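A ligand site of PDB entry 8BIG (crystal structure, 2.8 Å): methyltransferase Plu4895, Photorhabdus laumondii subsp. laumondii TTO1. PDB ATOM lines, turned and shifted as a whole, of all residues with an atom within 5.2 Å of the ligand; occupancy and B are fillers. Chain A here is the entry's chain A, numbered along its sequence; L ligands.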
ATOM      1  N   PHE A 127      30.873  24.228 -12.116  1.00  0.00           N
ATOM      2  CA  PHE A 127      29.387  24.226 -12.184  1.00  0.00           C
ATOM      3  C   PHE A 127      28.901  23.508 -13.448  1.00  0.00           C
ATOM      4  O   PHE A 127      27.779  22.978 -13.432  1.00  0.00           O
ATOM      5  CB  PHE A 127      28.842  25.658 -12.074  1.00  0.00           C
ATOM      6  CG  PHE A 127      28.948  26.243 -10.688  1.00  0.00           C
ATOM      7  CD1 PHE A 127      28.279  25.653  -9.627  1.00  0.00           C
ATOM      8  CD2 PHE A 127      29.731  27.361 -10.440  1.00  0.00           C
ATOM      9  CE1 PHE A 127      28.380  26.181  -8.347  1.00  0.00           C
ATOM     10  CE2 PHE A 127      29.819  27.885  -9.161  1.00  0.00           C
ATOM     11  CZ  PHE A 127      29.148  27.302  -8.116  1.00  0.00           C
ATOM     12  N   LYS A 137      25.763  17.309  -6.909  1.00  0.00           N
ATOM     13  CA  LYS A 137      25.022  18.606  -6.879  1.00  0.00           C
ATOM     14  C   LYS A 137      24.006  18.595  -5.734  1.00  0.00           C
ATOM     15  O   LYS A 137      23.832  19.642  -5.081  1.00  0.00           O
ATOM     16  CB  LYS A 137      24.306  18.873  -8.209  1.00  0.00           C
ATOM     17  CG  LYS A 137      23.936  20.334  -8.445  1.00  0.00           C
ATOM     18  CD  LYS A 137      22.535  20.537  -8.992  1.00  0.00           C
ATOM     19  CE  LYS A 137      22.281  21.960  -9.439  1.00  0.00           C
ATOM     20  NZ  LYS A 137      22.557  22.954  -8.370  1.00  0.00           N
ATOM     21  N   PHE A 140      26.043  19.067  -2.670  1.00  0.00           N
ATOM     22  CA  PHE A 140      26.509  20.483  -2.705  1.00  0.00           C
ATOM     23  C   PHE A 140      25.399  21.391  -2.154  1.00  0.00           C
ATOM     24  O   PHE A 140      25.661  22.139  -1.204  1.00  0.00           O
ATOM     25  CB  PHE A 140      26.911  20.888  -4.121  1.00  0.00           C
ATOM     26  CG  PHE A 140      27.271  22.348  -4.284  1.00  0.00           C
ATOM     27  CD1 PHE A 140      28.485  22.835  -3.834  1.00  0.00           C
ATOM     28  CD2 PHE A 140      26.389  23.229  -4.886  1.00  0.00           C
ATOM     29  CE1 PHE A 140      28.812  24.171  -3.980  1.00  0.00           C
ATOM     30  CE2 PHE A 140      26.720  24.577  -5.027  1.00  0.00           C
ATOM     31  CZ  PHE A 140      27.934  25.042  -4.580  1.00  0.00           C
ATOM     32  N   ASP A 141      24.199  21.299  -2.736  1.00  0.00           N
ATOM     33  CA  ASP A 141      23.010  22.121  -2.367  1.00  0.00           C
ATOM     34  C   ASP A 141      22.595  21.815  -0.919  1.00  0.00           C
ATOM     35  O   ASP A 141      22.119  22.754  -0.248  1.00  0.00           O
ATOM     36  CB  ASP A 141      21.845  21.886  -3.332  1.00  0.00           C
ATOM     37  CG  ASP A 141      22.046  22.478  -4.716  1.00  0.00           C
ATOM     38  OD1 ASP A 141      22.888  23.385  -4.851  1.00  0.00           O
ATOM     39  OD2 ASP A 141      21.353  22.019  -5.652  1.00  0.00           O
ATOM     40  N   MET A 144      24.965  23.657   1.336  1.00  0.00           N
ATOM     41  CA  MET A 144      24.692  25.109   1.164  1.00  0.00           C
ATOM     42  C   MET A 144      23.504  25.512   2.045  1.00  0.00           C
ATOM     43  O   MET A 144      23.572  26.600   2.661  1.00  0.00           O
ATOM     44  CB  MET A 144      24.387  25.442  -0.294  1.00  0.00           C
ATOM     45  CG  MET A 144      25.589  25.306  -1.205  1.00  0.00           C
ATOM     46  SD  MET A 144      26.853  26.559  -0.872  1.00  0.00           S
ATOM     47  CE  MET A 144      28.252  25.500  -0.503  1.00  0.00           C
ATOM     48  N   SER A 145      22.467  24.665   2.103  1.00  0.00           N
ATOM     49  CA  SER A 145      21.258  24.850   2.953  1.00  0.00           C
ATOM     50  C   SER A 145      21.658  25.024   4.423  1.00  0.00           C
ATOM     51  O   SER A 145      21.028  25.840   5.111  1.00  0.00           O
ATOM     52  CB  SER A 145      20.315  23.678   2.804  1.00  0.00           C
ATOM     53  OG  SER A 145      20.055  23.411   1.432  1.00  0.00           O
ATOM     54  N   THR A 148      23.210  28.335   4.994  1.00  0.00           N
ATOM     55  CA  THR A 148      22.041  29.244   4.880  1.00  0.00           C
ATOM     56  C   THR A 148      21.306  29.296   6.236  1.00  0.00           C
ATOM     57  O   THR A 148      20.964  30.411   6.662  1.00  0.00           O
ATOM     58  CB  THR A 148      21.101  28.822   3.743  1.00  0.00           C
ATOM     59  OG1 THR A 148      21.754  29.078   2.499  1.00  0.00           O
ATOM     60  CG2 THR A 148      19.767  29.535   3.774  1.00  0.00           C
ATOM     61  N   ASP A 169      16.642  36.285  -5.941  1.00  0.00           N
ATOM     62  CA  ASP A 169      17.889  35.661  -5.412  1.00  0.00           C
ATOM     63  C   ASP A 169      18.714  35.147  -6.606  1.00  0.00           C
ATOM     64  O   ASP A 169      18.349  34.089  -7.176  1.00  0.00           O
ATOM     65  CB  ASP A 169      17.568  34.551  -4.408  1.00  0.00           C
ATOM     66  CG  ASP A 169      18.770  34.016  -3.640  1.00  0.00           C
ATOM     67  OD1 ASP A 169      19.879  34.532  -3.856  1.00  0.00           O
ATOM     68  OD2 ASP A 169      18.570  33.088  -2.833  1.00  0.00           O
ATOM     69  N   GLY A 171      21.613  33.284  -8.392  1.00  0.00           N
ATOM     70  CA  GLY A 171      22.360  32.056  -8.050  1.00  0.00           C
ATOM     71  C   GLY A 171      21.922  31.507  -6.701  1.00  0.00           C
ATOM     72  O   GLY A 171      22.799  31.188  -5.871  1.00  0.00           O
ATOM     73  N   GLY A 172      20.603  31.427  -6.482  1.00  0.00           N
ATOM     74  CA  GLY A 172      19.996  30.989  -5.201  1.00  0.00           C
ATOM     75  C   GLY A 172      19.930  29.482  -5.060  1.00  0.00           C
ATOM     76  O   GLY A 172      19.651  29.012  -3.943  1.00  0.00           O
ATOM     77  N   GLY A 173      20.182  28.745  -6.153  1.00  0.00           N
ATOM     78  CA  GLY A 173      20.078  27.271  -6.202  1.00  0.00           C
ATOM     79  C   GLY A 173      18.664  26.818  -5.867  1.00  0.00           C
ATOM     80  O   GLY A 173      17.723  27.386  -6.436  1.00  0.00           O
ATOM     81  N   LEU A 193      16.680  32.794  -9.268  1.00  0.00           N
ATOM     82  CA  LEU A 193      17.293  32.639 -10.614  1.00  0.00           C
ATOM     83  C   LEU A 193      18.560  31.787 -10.484  1.00  0.00           C
ATOM     84  O   LEU A 193      19.418  32.131  -9.640  1.00  0.00           O
ATOM     85  CB  LEU A 193      17.609  34.018 -11.195  1.00  0.00           C
ATOM     86  CG  LEU A 193      18.094  34.036 -12.643  1.00  0.00           C
ATOM     87  CD1 LEU A 193      17.603  35.280 -13.362  1.00  0.00           C
ATOM     88  CD2 LEU A 193      19.610  33.931 -12.727  1.00  0.00           C
ATOM     89  N   ASP A 194      18.683  30.723 -11.292  1.00  0.00           N
ATOM     90  CA  ASP A 194      19.828  29.786 -11.270  1.00  0.00           C
ATOM     91  C   ASP A 194      19.777  28.866 -12.498  1.00  0.00           C
ATOM     92  O   ASP A 194      18.727  28.808 -13.162  1.00  0.00           O
ATOM     93  CB  ASP A 194      19.833  28.963  -9.980  1.00  0.00           C
ATOM     94  CG  ASP A 194      21.216  28.482  -9.546  1.00  0.00           C
ATOM     95  OD1 ASP A 194      21.859  27.777 -10.339  1.00  0.00           O
ATOM     96  OD2 ASP A 194      21.621  28.831  -8.424  1.00  0.00           O
ATOM     97  N   ARG A 195      20.897  28.182 -12.769  1.00  0.00           N
ATOM     98  CA  ARG A 195      21.044  27.158 -13.833  1.00  0.00           C
ATOM     99  C   ARG A 195      20.406  25.841 -13.365  1.00  0.00           C
ATOM    100  O   ARG A 195      21.035  25.136 -12.549  1.00  0.00           O
ATOM    101  CB  ARG A 195      22.532  26.944 -14.183  1.00  0.00           C
ATOM    102  CG  ARG A 195      23.459  26.872 -12.978  1.00  0.00           C
ATOM    103  CD  ARG A 195      24.730  26.072 -13.218  1.00  0.00           C
ATOM    104  NE  ARG A 195      25.776  26.898 -13.805  1.00  0.00           N
ATOM    105  CZ  ARG A 195      26.350  26.677 -14.992  1.00  0.00           C
ATOM    106  NH1 ARG A 195      27.297  27.504 -15.419  1.00  0.00           N
ATOM    107  NH2 ARG A 195      26.006  25.653 -15.746  1.00  0.00           N
ATOM    108  N   GLY A 210      17.883  30.906 -15.643  1.00  0.00           N
ATOM    109  CA  GLY A 210      18.617  32.111 -16.080  1.00  0.00           C
ATOM    110  C   GLY A 210      20.124  31.991 -15.917  1.00  0.00           C
ATOM    111  O   GLY A 210      20.586  31.036 -15.258  1.00  0.00           O
ATOM    112  N   ASP A 211      20.847  32.954 -16.516  1.00  0.00           N
ATOM    113  CA  ASP A 211      22.320  33.141 -16.416  1.00  0.00           C
ATOM    114  C   ASP A 211      22.573  34.604 -16.044  1.00  0.00           C
ATOM    115  O   ASP A 211      22.200  35.479 -16.859  1.00  0.00           O
ATOM    116  CB  ASP A 211      22.992  32.743 -17.735  1.00  0.00           C
ATOM    117  CG  ASP A 211      24.494  33.005 -17.789  1.00  0.00           C
ATOM    118  OD1 ASP A 211      25.024  33.051 -18.919  1.00  0.00           O
ATOM    119  OD2 ASP A 211      25.106  33.153 -16.724  1.00  0.00           O
ATOM    120  N   PHE A 212      23.168  34.873 -14.886  1.00  0.00           N
ATOM    121  CA  PHE A 212      23.374  36.246 -14.352  1.00  0.00           C
ATOM    122  C   PHE A 212      24.486  36.979 -15.126  1.00  0.00           C
ATOM    123  O   PHE A 212      24.709  38.175 -14.849  1.00  0.00           O
ATOM    124  CB  PHE A 212      23.623  36.261 -12.837  1.00  0.00           C
ATOM    125  CG  PHE A 212      24.653  35.310 -12.293  1.00  0.00           C
ATOM    126  CD1 PHE A 212      25.903  35.173 -12.872  1.00  0.00           C
ATOM    127  CD2 PHE A 212      24.383  34.569 -11.151  1.00  0.00           C
ATOM    128  CE1 PHE A 212      26.841  34.296 -12.344  1.00  0.00           C
ATOM    129  CE2 PHE A 212      25.324  33.704 -10.617  1.00  0.00           C
ATOM    130  CZ  PHE A 212      26.553  33.566 -11.221  1.00  0.00           C
ATOM    131  N   PHE A 213      25.168  36.291 -16.054  1.00  0.00           N
ATOM    132  CA  PHE A 213      26.134  36.892 -17.017  1.00  0.00           C
ATOM    133  C   PHE A 213      25.351  37.539 -18.174  1.00  0.00           C
ATOM    134  O   PHE A 213      25.938  38.393 -18.872  1.00  0.00           O
ATOM    135  CB  PHE A 213      27.140  35.843 -17.513  1.00  0.00           C
ATOM    136  CG  PHE A 213      28.225  35.521 -16.521  1.00  0.00           C
ATOM    137  CD1 PHE A 213      29.144  36.485 -16.143  1.00  0.00           C
ATOM    138  CD2 PHE A 213      28.329  34.255 -15.960  1.00  0.00           C
ATOM    139  CE1 PHE A 213      30.142  36.192 -15.231  1.00  0.00           C
ATOM    140  CE2 PHE A 213      29.327  33.961 -15.047  1.00  0.00           C
ATOM    141  CZ  PHE A 213      30.236  34.932 -14.679  1.00  0.00           C
ATOM    142  N   LYS A 226      24.188  35.890  -2.567  1.00  0.00           N
ATOM    143  CA  LYS A 226      24.733  35.169  -1.389  1.00  0.00           C
ATOM    144  C   LYS A 226      25.645  34.039  -1.868  1.00  0.00           C
ATOM    145  O   LYS A 226      25.133  33.124  -2.552  1.00  0.00           O
ATOM    146  CB  LYS A 226      23.603  34.624  -0.513  1.00  0.00           C
ATOM    147  CG  LYS A 226      24.066  33.792   0.674  1.00  0.00           C
ATOM    148  CD  LYS A 226      22.938  33.226   1.503  1.00  0.00           C
ATOM    149  CE  LYS A 226      23.408  32.209   2.513  1.00  0.00           C
ATOM    150  NZ  LYS A 226      23.589  30.874   1.911  1.00  0.00           N
ATOM    151  N   ASN A 227      26.925  34.089  -1.508  1.00  0.00           N
ATOM    152  CA  ASN A 227      27.957  33.063  -1.832  1.00  0.00           C
ATOM    153  C   ASN A 227      28.030  32.854  -3.347  1.00  0.00           C
ATOM    154  O   ASN A 227      28.027  31.677  -3.782  1.00  0.00           O
ATOM    155  CB  ASN A 227      27.679  31.730  -1.138  1.00  0.00           C
ATOM    156  CG  ASN A 227      27.928  31.772   0.350  1.00  0.00           C
ATOM    157  OD1 ASN A 227      28.906  32.354   0.807  1.00  0.00           O
ATOM    158  ND2 ASN A 227      27.055  31.128   1.122  1.00  0.00           N
ATOM    159  N   VAL A 228      28.080  33.931  -4.132  1.00  0.00           N
ATOM    160  CA  VAL A 228      28.199  33.863  -5.616  1.00  0.00           C
ATOM    161  C   VAL A 228      29.520  34.498  -6.059  1.00  0.00           C
ATOM    162  O   VAL A 228      30.239  33.852  -6.846  1.00  0.00           O
ATOM    163  CB  VAL A 228      26.971  34.503  -6.304  1.00  0.00           C
ATOM    164  CG1 VAL A 228      27.200  34.727  -7.796  1.00  0.00           C
ATOM    165  CG2 VAL A 228      25.716  33.671  -6.080  1.00  0.00           C
ATOM    166  N   ASN A 231      32.955  32.806  -6.143  1.00  0.00           N
ATOM    167  CA  ASN A 231      33.113  31.767  -7.196  1.00  0.00           C
ATOM    168  C   ASN A 231      33.708  32.371  -8.478  1.00  0.00           C
ATOM    169  O   ASN A 231      33.926  31.598  -9.432  1.00  0.00           O
ATOM    170  CB  ASN A 231      31.785  31.098  -7.564  1.00  0.00           C
ATOM    171  CG  ASN A 231      31.111  30.398  -6.405  1.00  0.00           C
ATOM    172  OD1 ASN A 231      31.759  30.022  -5.433  1.00  0.00           O
ATOM    173  ND2 ASN A 231      29.804  30.210  -6.513  1.00  0.00           N
ATOM    174  N   TRP A 232      33.937  33.694  -8.526  1.00  0.00           N
ATOM    175  CA  TRP A 232      34.251  34.414  -9.789  1.00  0.00           C
ATOM    176  C   TRP A 232      35.458  35.336  -9.608  1.00  0.00           C
ATOM    177  O   TRP A 232      35.589  35.994  -8.579  1.00  0.00           O
ATOM    178  CB  TRP A 232      33.019  35.181 -10.275  1.00  0.00           C
ATOM    179  CG  TRP A 232      31.846  34.274 -10.490  1.00  0.00           C
ATOM    180  CD1 TRP A 232      30.711  34.202  -9.753  1.00  0.00           C
ATOM    181  CD2 TRP A 232      31.738  33.242 -11.497  1.00  0.00           C
ATOM    182  NE1 TRP A 232      29.878  33.223 -10.233  1.00  0.00           N
ATOM    183  CE2 TRP A 232      30.488  32.619 -11.307  1.00  0.00           C
ATOM    184  CE3 TRP A 232      32.565  32.803 -12.537  1.00  0.00           C
ATOM    185  CZ2 TRP A 232      30.051  31.572 -12.126  1.00  0.00           C
ATOM    186  CZ3 TRP A 232      32.126  31.780 -13.339  1.00  0.00           C
ATOM    187  CH2 TRP A 232      30.885  31.174 -13.137  1.00  0.00           C
HETATM  188  N1  LIG L   1      23.219  31.112  -2.811  1.00  0.00           N
HETATM  189  C1  LIG L   1      23.200  29.641  -2.518  1.00  0.00           C
HETATM  190  C2  LIG L   1      24.397  28.875  -3.097  1.00  0.00           C
HETATM  191  C3  LIG L   1      25.209  29.650  -4.116  1.00  0.00           C
HETATM  192  S1  LIG L   1      26.678  28.739  -4.638  1.00  0.00           S
HETATM  193  C4  LIG L   1      23.195  29.434  -0.995  1.00  0.00           C
HETATM  194  O1  LIG L   1      22.355  28.734  -0.441  1.00  0.00           O
HETATM  195  O2  LIG L   1      24.051  29.982  -0.302  1.00  0.00           O
HETATM  196  C5  LIG L   1      26.765  29.160  -6.397  1.00  0.00           C
HETATM  197  C6  LIG L   1      25.436  29.118  -7.104  1.00  0.00           C
HETATM  198  O3  LIG L   1      25.504  29.910  -8.300  1.00  0.00           O
HETATM  199  C7  LIG L   1      24.986  27.717  -7.539  1.00  0.00           C
HETATM  200  O4  LIG L   1      23.623  27.479  -7.183  1.00  0.00           O
HETATM  201  C8  LIG L   1      25.170  27.750  -9.054  1.00  0.00           C
HETATM  202  O5  LIG L   1      24.293  26.893  -9.748  1.00  0.00           O
HETATM  203  C9  LIG L   1      24.853  29.218  -9.335  1.00  0.00           C
HETATM  204  N2  LIG L   1      25.349  29.716 -10.611  1.00  0.00           N
HETATM  205  C10 LIG L   1      26.573  29.478 -11.176  1.00  0.00           C
HETATM  206  N3  LIG L   1      26.733  30.083 -12.330  1.00  0.00           N
HETATM  207  C11 LIG L   1      25.538  30.762 -12.530  1.00  0.00           C
HETATM  208  C12 LIG L   1      25.085  31.582 -13.583  1.00  0.00           C
HETATM  209  N4  LIG L   1      25.805  31.876 -14.653  1.00  0.00           N
HETATM  210  N5  LIG L   1      23.841  32.107 -13.466  1.00  0.00           N
HETATM  211  C13 LIG L   1      23.110  31.803 -12.382  1.00  0.00           C
HETATM  212  N6  LIG L   1      23.436  31.045 -11.339  1.00  0.00           N
HETATM  213  C14 LIG L   1      24.673  30.546 -11.476  1.00  0.00           C
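O of Asn 227 lies close to S1 of the ligand, at 3.3 Å.
CZ of Phe 127 touches C5 of the ligand, 3.5 Å away.
Phe 140 touches the ligand.
Met 144 touches the ligand.
O of Gly 172 touches C1 of the ligand, at 3.9 Å.
CA of Gly 173 touches O4 of the ligand, at 3.7 Å.
CG of Arg 195 touches O5 of the ligand (3.3 Å).
Gly 210 touches the ligand.
Phe 213 touches the ligand.
Asn 231 touches the ligand.
Trp 232 touches the ligand (CZ2 to N3, 3.6 Å).
Within 4 Å of the ligand: Phe 127, Phe 140, Met 144, Thr 148, Gly 171, Gly 172, Gly 173, Asp 194, Arg 195, Gly 210, Asp 211, Phe 212, Phe 213, Lys 226, Asn 227, Asn 231 and Trp 232.
The nearest printed residue that does not touch the ligand is Leu 193 (4.1 Å).
The backbone carbonyl oxygen of Lys 226 lies within hydrogen-bond range of a nitrogen (N1) of the ligand, at 2.8 Å.
NZ of Lys 226 lies within salt-bridge range of O2 of the ligand, at 2.4 Å.
A nitrogen (N4) of the ligand is in hydrogen-bond range of the side-chain carboxylate (OD2) of Asp 211 (2.5 Å).
OD1 of Asp 194 is in hydrogen-bond range of O5 of the ligand (2.7 Å).
An oxygen (O1) of the ligand is in hydrogen-bond range of the side-chain hydroxyl of Thr 148.
A nitrogen (N1) of the ligand is in hydrogen-bond range of the backbone carbonyl oxygen of Gly 171.
The backbone NH (N) of Phe 212 is in hydrogen-bond range of a nitrogen (N5) of the ligand.
The side-chain amino group (NZ) of Lys 226 lies within hydrogen-bond range of the side-chain hydroxyl (OG1) of Thr 148, 2.6 Å away.
The side-chain carboxylate (OD2) of Asp 194 lies within hydrogen-bond range of the backbone NH (N) of Gly 173 (2.7 Å).
The backbone carbonyl oxygen (O) of Asp 194 lies within hydrogen-bond range of the backbone NH (N) of Gly 210, 3.4 Å away.
OD2 of Asp 194 is in hydrogen-bond range of N of Gly 172 (3.4 Å).
The side-chain hydroxyl (OG1) of Thr 148 is in hydrogen-bond range of the backbone carbonyl oxygen (O) of Met 144, 3.1 Å away.
N of Gly 171 sits at hydrogen-bond distance from O of Leu 193 (2.8 Å).
The indole nitrogen (NE1) of Trp 232 lies close to the backbone carbonyl oxygen (O) of Val 228, 3.5 Å away.
The backbone NH (N) of Gly 172 sits at hydrogen-bond distance from the backbone carbonyl oxygen (O) of Leu 193, at 3.4 Å.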
